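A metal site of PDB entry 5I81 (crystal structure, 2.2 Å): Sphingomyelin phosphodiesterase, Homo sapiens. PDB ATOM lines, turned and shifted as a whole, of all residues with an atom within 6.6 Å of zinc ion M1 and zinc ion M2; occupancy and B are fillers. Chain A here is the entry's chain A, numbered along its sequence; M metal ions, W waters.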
ATOM      1  N   THR A 159     -22.542 -22.313 -32.903  1.00  0.00           N
ATOM      2  CA  THR A 159     -22.860 -22.135 -31.494  1.00  0.00           C
ATOM      3  C   THR A 159     -22.592 -20.696 -31.068  1.00  0.00           C
ATOM      4  O   THR A 159     -21.740 -19.997 -31.643  1.00  0.00           O
ATOM      5  CB  THR A 159     -22.083 -23.139 -30.631  1.00  0.00           C
ATOM      6  OG1 THR A 159     -22.593 -23.125 -29.300  1.00  0.00           O
ATOM      7  CG2 THR A 159     -20.590 -22.829 -30.623  1.00  0.00           C
ATOM      8  N   ASP A 160     -23.355 -20.229 -30.076  1.00  0.00           N
ATOM      9  CA  ASP A 160     -23.158 -18.900 -29.509  1.00  0.00           C
ATOM     10  C   ASP A 160     -23.141 -17.822 -30.594  1.00  0.00           C
ATOM     11  O   ASP A 160     -22.168 -17.078 -30.778  1.00  0.00           O
ATOM     12  CB  ASP A 160     -21.895 -18.864 -28.639  1.00  0.00           C
ATOM     13  CG  ASP A 160     -21.919 -19.952 -27.570  1.00  0.00           C
ATOM     14  OD1 ASP A 160     -22.510 -19.661 -26.492  1.00  0.00           O
ATOM     15  OD2 ASP A 160     -21.430 -21.079 -27.790  1.00  0.00           O
ATOM     16  N   LEU A 161     -24.265 -17.755 -31.310  1.00  0.00           N
ATOM     17  CA  LEU A 161     -24.390 -16.762 -32.369  1.00  0.00           C
ATOM     18  C   LEU A 161     -24.589 -15.355 -31.781  1.00  0.00           C
ATOM     19  O   LEU A 161     -24.065 -14.384 -32.315  1.00  0.00           O
ATOM     20  CB  LEU A 161     -25.521 -17.150 -33.324  1.00  0.00           C
ATOM     21  CG  LEU A 161     -25.182 -18.130 -34.472  1.00  0.00           C
ATOM     22  CD1 LEU A 161     -24.471 -19.457 -34.014  1.00  0.00           C
ATOM     23  CD2 LEU A 161     -26.473 -18.434 -35.202  1.00  0.00           C
ATOM     24  N   HIS A 162     -25.330 -15.242 -30.676  1.00  0.00           N
ATOM     25  CA  HIS A 162     -25.489 -13.978 -29.932  1.00  0.00           C
ATOM     26  C   HIS A 162     -25.780 -12.769 -30.838  1.00  0.00           C
ATOM     27  O   HIS A 162     -25.035 -11.774 -30.870  1.00  0.00           O
ATOM     28  CB  HIS A 162     -24.253 -13.697 -29.075  1.00  0.00           C
ATOM     29  CG  HIS A 162     -24.196 -14.541 -27.846  1.00  0.00           C
ATOM     30  ND1 HIS A 162     -23.247 -15.523 -27.666  1.00  0.00           N
ATOM     31  CD2 HIS A 162     -24.994 -14.571 -26.749  1.00  0.00           C
ATOM     32  CE1 HIS A 162     -23.441 -16.093 -26.493  1.00  0.00           C
ATOM     33  NE2 HIS A 162     -24.507 -15.548 -25.925  1.00  0.00           N
ATOM     34  N   GLY A 231     -26.969 -23.391 -29.224  1.00  0.00           N
ATOM     35  CA  GLY A 231     -27.531 -22.477 -28.246  1.00  0.00           C
ATOM     36  C   GLY A 231     -26.837 -21.121 -28.180  1.00  0.00           C
ATOM     37  O   GLY A 231     -25.727 -20.918 -28.681  1.00  0.00           O
ATOM     38  N   ASP A 232     -27.560 -20.197 -27.524  1.00  0.00           N
ATOM     39  CA  ASP A 232     -27.231 -18.784 -27.270  1.00  0.00           C
ATOM     40  C   ASP A 232     -27.535 -17.933 -28.504  1.00  0.00           C
ATOM     41  O   ASP A 232     -26.629 -17.584 -29.261  1.00  0.00           O
ATOM     42  CB  ASP A 232     -25.791 -18.606 -26.847  1.00  0.00           C
ATOM     43  CG  ASP A 232     -25.592 -18.695 -25.331  1.00  0.00           C
ATOM     44  OD1 ASP A 232     -26.502 -19.097 -24.562  1.00  0.00           O
ATOM     45  OD2 ASP A 232     -24.454 -18.352 -24.920  1.00  0.00           O
ATOM     46  N   HIS A 236     -25.707 -10.305 -25.133  1.00  0.00           N
ATOM     47  CA  HIS A 236     -25.423 -10.142 -23.705  1.00  0.00           C
ATOM     48  C   HIS A 236     -26.016  -8.858 -23.127  1.00  0.00           C
ATOM     49  O   HIS A 236     -25.555  -8.395 -22.075  1.00  0.00           O
ATOM     50  CB  HIS A 236     -23.913 -10.193 -23.450  1.00  0.00           C
ATOM     51  CG  HIS A 236     -23.267 -11.500 -23.843  1.00  0.00           C
ATOM     52  ND1 HIS A 236     -23.011 -11.833 -25.162  1.00  0.00           N
ATOM     53  CD2 HIS A 236     -22.864 -12.564 -23.092  1.00  0.00           C
ATOM     54  CE1 HIS A 236     -22.480 -13.047 -25.202  1.00  0.00           C
ATOM     55  NE2 HIS A 236     -22.375 -13.511 -23.967  1.00  0.00           N
ATOM     56  N   GLY A 271     -29.396 -22.801 -25.104  1.00  0.00           N
ATOM     57  CA  GLY A 271     -28.318 -22.090 -24.432  1.00  0.00           C
ATOM     58  C   GLY A 271     -28.810 -21.413 -23.171  1.00  0.00           C
ATOM     59  O   GLY A 271     -30.013 -21.387 -22.900  1.00  0.00           O
ATOM     60  N   ASN A 272     -27.864 -20.861 -22.390  1.00  0.00           N
ATOM     61  CA  ASN A 272     -28.248 -20.179 -21.164  1.00  0.00           C
ATOM     62  C   ASN A 272     -28.800 -18.780 -21.418  1.00  0.00           C
ATOM     63  O   ASN A 272     -29.376 -18.192 -20.495  1.00  0.00           O
ATOM     64  CB  ASN A 272     -27.051 -20.100 -20.194  1.00  0.00           C
ATOM     65  CG  ASN A 272     -25.866 -19.379 -20.794  1.00  0.00           C
ATOM     66  OD1 ASN A 272     -25.397 -19.717 -21.890  1.00  0.00           O
ATOM     67  ND2 ASN A 272     -25.376 -18.343 -20.086  1.00  0.00           N
ATOM     68  N   HIS A 273     -28.683 -18.236 -22.631  1.00  0.00           N
ATOM     69  CA  HIS A 273     -29.158 -16.890 -22.906  1.00  0.00           C
ATOM     70  C   HIS A 273     -30.529 -16.855 -23.550  1.00  0.00           C
ATOM     71  O   HIS A 273     -31.055 -15.754 -23.780  1.00  0.00           O
ATOM     72  CB  HIS A 273     -28.177 -16.108 -23.780  1.00  0.00           C
ATOM     73  CG  HIS A 273     -27.030 -15.525 -23.013  1.00  0.00           C
ATOM     74  ND1 HIS A 273     -27.004 -14.212 -22.620  1.00  0.00           N
ATOM     75  CD2 HIS A 273     -25.859 -16.082 -22.573  1.00  0.00           C
ATOM     76  CE1 HIS A 273     -25.889 -13.982 -21.946  1.00  0.00           C
ATOM     77  NE2 HIS A 273     -25.185 -15.089 -21.900  1.00  0.00           N
ATOM     78  N   ASN A 279     -30.021 -17.133 -17.812  1.00  0.00           N
ATOM     79  CA  ASN A 279     -29.819 -18.297 -16.937  1.00  0.00           C
ATOM     80  C   ASN A 279     -31.060 -18.738 -16.159  1.00  0.00           C
ATOM     81  O   ASN A 279     -30.967 -19.687 -15.345  1.00  0.00           O
ATOM     82  CB  ASN A 279     -28.682 -18.076 -15.911  1.00  0.00           C
ATOM     83  CG  ASN A 279     -27.354 -17.655 -16.571  1.00  0.00           C
ATOM     84  OD1 ASN A 279     -26.782 -16.620 -16.203  1.00  0.00           O
ATOM     85  ND2 ASN A 279     -26.869 -18.436 -17.531  1.00  0.00           N
ATOM     86  N   HIS A 379     -25.044 -27.181 -24.524  1.00  0.00           N
ATOM     87  CA  HIS A 379     -24.460 -25.860 -24.503  1.00  0.00           C
ATOM     88  C   HIS A 379     -23.334 -25.753 -23.485  1.00  0.00           C
ATOM     89  O   HIS A 379     -22.159 -25.779 -23.860  1.00  0.00           O
ATOM     90  CB  HIS A 379     -25.550 -24.819 -24.221  1.00  0.00           C
ATOM     91  CG  HIS A 379     -25.059 -23.420 -24.316  1.00  0.00           C
ATOM     92  ND1 HIS A 379     -24.664 -22.855 -25.505  1.00  0.00           N
ATOM     93  CD2 HIS A 379     -24.838 -22.490 -23.351  1.00  0.00           C
ATOM     94  CE1 HIS A 379     -24.231 -21.624 -25.274  1.00  0.00           C
ATOM     95  NE2 HIS A 379     -24.343 -21.386 -23.976  1.00  0.00           N
ATOM     96  N   ILE A 380     -23.673 -25.602 -22.201  1.00  0.00           N
ATOM     97  CA  ILE A 380     -22.640 -25.530 -21.147  1.00  0.00           C
ATOM     98  C   ILE A 380     -21.866 -26.846 -21.116  1.00  0.00           C
ATOM     99  O   ILE A 380     -22.500 -27.914 -20.980  1.00  0.00           O
ATOM    100  CB  ILE A 380     -23.290 -25.248 -19.786  1.00  0.00           C
ATOM    101  CG1 ILE A 380     -24.074 -23.926 -19.804  1.00  0.00           C
ATOM    102  CG2 ILE A 380     -22.275 -25.341 -18.664  1.00  0.00           C
ATOM    103  CD1 ILE A 380     -24.938 -23.678 -18.573  1.00  0.00           C
ATOM    104  N   GLY A 410     -20.647 -26.011 -26.294  1.00  0.00           N
ATOM    105  CA  GLY A 410     -20.254 -24.660 -26.648  1.00  0.00           C
ATOM    106  C   GLY A 410     -20.035 -23.826 -25.402  1.00  0.00           C
ATOM    107  O   GLY A 410     -19.294 -24.225 -24.485  1.00  0.00           O
ATOM    108  N   HIS A 411     -20.667 -22.648 -25.386  1.00  0.00           N
ATOM    109  CA  HIS A 411     -20.792 -21.797 -24.201  1.00  0.00           C
ATOM    110  C   HIS A 411     -19.513 -21.040 -23.821  1.00  0.00           C
ATOM    111  O   HIS A 411     -19.632 -19.858 -23.483  1.00  0.00           O
ATOM    112  CB  HIS A 411     -21.265 -22.593 -22.978  1.00  0.00           C
ATOM    113  CG  HIS A 411     -21.428 -21.767 -21.735  1.00  0.00           C
ATOM    114  ND1 HIS A 411     -22.359 -20.756 -21.625  1.00  0.00           N
ATOM    115  CD2 HIS A 411     -20.812 -21.844 -20.525  1.00  0.00           C
ATOM    116  CE1 HIS A 411     -22.292 -20.228 -20.417  1.00  0.00           C
ATOM    117  NE2 HIS A 411     -21.364 -20.874 -19.729  1.00  0.00           N
ATOM    118  N   THR A 412     -18.309 -21.651 -23.879  1.00  0.00           N
ATOM    119  CA  THR A 412     -17.120 -20.876 -23.461  1.00  0.00           C
ATOM    120  C   THR A 412     -16.621 -19.926 -24.543  1.00  0.00           C
ATOM    121  O   THR A 412     -15.812 -19.054 -24.251  1.00  0.00           O
ATOM    122  CB  THR A 412     -15.940 -21.790 -23.052  1.00  0.00           C
ATOM    123  OG1 THR A 412     -15.421 -22.467 -24.210  1.00  0.00           O
ATOM    124  CG2 THR A 412     -16.371 -22.841 -22.044  1.00  0.00           C
ATOM    125  N   HIS A 413     -17.051 -20.090 -25.783  1.00  0.00           N
ATOM    126  CA  HIS A 413     -16.732 -19.219 -26.916  1.00  0.00           C
ATOM    127  C   HIS A 413     -15.317 -19.416 -27.453  1.00  0.00           C
ATOM    128  O   HIS A 413     -15.012 -18.867 -28.505  1.00  0.00           O
ATOM    129  CB  HIS A 413     -16.925 -17.709 -26.629  1.00  0.00           C
ATOM    130  CG  HIS A 413     -18.342 -17.302 -26.360  1.00  0.00           C
ATOM    131  ND1 HIS A 413     -18.731 -15.982 -26.309  1.00  0.00           N
ATOM    132  CD2 HIS A 413     -19.457 -18.032 -26.151  1.00  0.00           C
ATOM    133  CE1 HIS A 413     -20.028 -15.913 -26.027  1.00  0.00           C
ATOM    134  NE2 HIS A 413     -20.492 -17.145 -25.941  1.00  0.00           N
ATOM    135  N   SER A 438     -17.112 -19.627 -30.671  1.00  0.00           N
ATOM    136  CA  SER A 438     -18.395 -18.958 -30.899  1.00  0.00           C
ATOM    137  C   SER A 438     -18.444 -18.235 -32.240  1.00  0.00           C
ATOM    138  O   SER A 438     -17.425 -17.773 -32.776  1.00  0.00           O
ATOM    139  CB  SER A 438     -18.684 -17.949 -29.778  1.00  0.00           C
ATOM    140  OG  SER A 438     -17.661 -16.959 -29.729  1.00  0.00           O
ATOM    141  N   THR A 440     -20.014 -15.476 -32.264  1.00  0.00           N
ATOM    142  CA  THR A 440     -19.884 -14.087 -31.823  1.00  0.00           C
ATOM    143  C   THR A 440     -18.434 -13.715 -31.547  1.00  0.00           C
ATOM    144  O   THR A 440     -17.583 -14.563 -31.252  1.00  0.00           O
ATOM    145  CB  THR A 440     -20.684 -13.796 -30.546  1.00  0.00           C
ATOM    146  OG1 THR A 440     -20.604 -12.396 -30.284  1.00  0.00           O
ATOM    147  CG2 THR A 440     -20.100 -14.574 -29.298  1.00  0.00           C
ATOM    148  N   TYR A 442     -17.781 -11.830 -28.907  1.00  0.00           N
ATOM    149  CA  TYR A 442     -17.725 -11.634 -27.460  1.00  0.00           C
ATOM    150  C   TYR A 442     -16.847 -12.660 -26.763  1.00  0.00           C
ATOM    151  O   TYR A 442     -17.185 -13.859 -26.801  1.00  0.00           O
ATOM    152  CB  TYR A 442     -19.158 -11.740 -26.891  1.00  0.00           C
ATOM    153  CG  TYR A 442     -19.323 -11.319 -25.427  1.00  0.00           C
ATOM    154  CD1 TYR A 442     -19.653 -10.000 -25.082  1.00  0.00           C
ATOM    155  CD2 TYR A 442     -19.206 -12.259 -24.387  1.00  0.00           C
ATOM    156  CE1 TYR A 442     -19.820  -9.614 -23.734  1.00  0.00           C
ATOM    157  CE2 TYR A 442     -19.371 -11.885 -23.033  1.00  0.00           C
ATOM    158  CZ  TYR A 442     -19.674 -10.569 -22.735  1.00  0.00           C
ATOM    159  OH  TYR A 442     -19.844 -10.209 -21.431  1.00  0.00           O
HETATM  160 ZN    ZN M   1     -23.608 -19.638 -23.083  1.00  0.00          ZN
HETATM  161 ZN    ZN M   2     -22.402 -17.712 -25.490  1.00  0.00          ZN
HETATM  162  O   HOH W   1     -22.236 -18.362 -23.228  1.00  0.00           O
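NE2 of His 413 is bound to zinc ion M2, at 2.0 Å. Zinc ion M2 is bound by the side-chain carboxylate (OD1) of Asp 160 (2.2 Å). OD2 of Asp 232 is bound to zinc ion M2 (2.2 Å). Water W1 binds zinc ion M2, 2.4 Å away.
Within 4 Å of zinc ion M1: Asp 160, Asp 232, Asn 272, His 379 and His 411. The nearest printed residue that does not touch zinc ion M1 is His 273 (4.2 Å).
The backbone carbonyl oxygen of His 413 sits at hydrogen-bond distance from the backbone NH of Ser 438, 3.1 Å away. The backbone carbonyl oxygen of His 379 lies within hydrogen-bond range of the backbone NH of Gly 410 (2.9 Å). The backbone carbonyl oxygen (O) of Asn 272 sits at hydrogen-bond distance from the backbone NH (N) of Asn 279 (3.0 Å). The backbone NH (N) of His 162 lies within hydrogen-bond range of the backbone carbonyl oxygen (O) of Asp 232 (3.0 Å). The backbone carbonyl oxygen of Asp 160 lies within hydrogen-bond range of the backbone NH of Thr 440 (3.1 Å). The backbone NH of Asp 160 lies within hydrogen-bond range of the backbone carbonyl oxygen of Gly 231, at 2.8 Å. The side-chain carboxylate (OD1) of Asp 232 is in hydrogen-bond range of the backbone NH (N) of His 273, 3.0 Å away. O of Asp 232 is in hydrogen-bond range of N of Leu 161 (3.1 Å).
CE1 of His 162 touches zinc ion M2 (2.2 Å). Within 4 Å of zinc ion M2: Asp 160, His 162, Asp 232 and His 413. The nearest printed residue that does not touch zinc ion M2 is His 411 (4.04 Å).
Zinc ion M1 is bound by water W1 (1.9 Å), NE2 of His 379 (2.1 Å), OD1 of Asn 272 (2.2 Å), ND1 of His 411 (2.2 Å) and OD2 of Asp 232 (2.4 Å).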
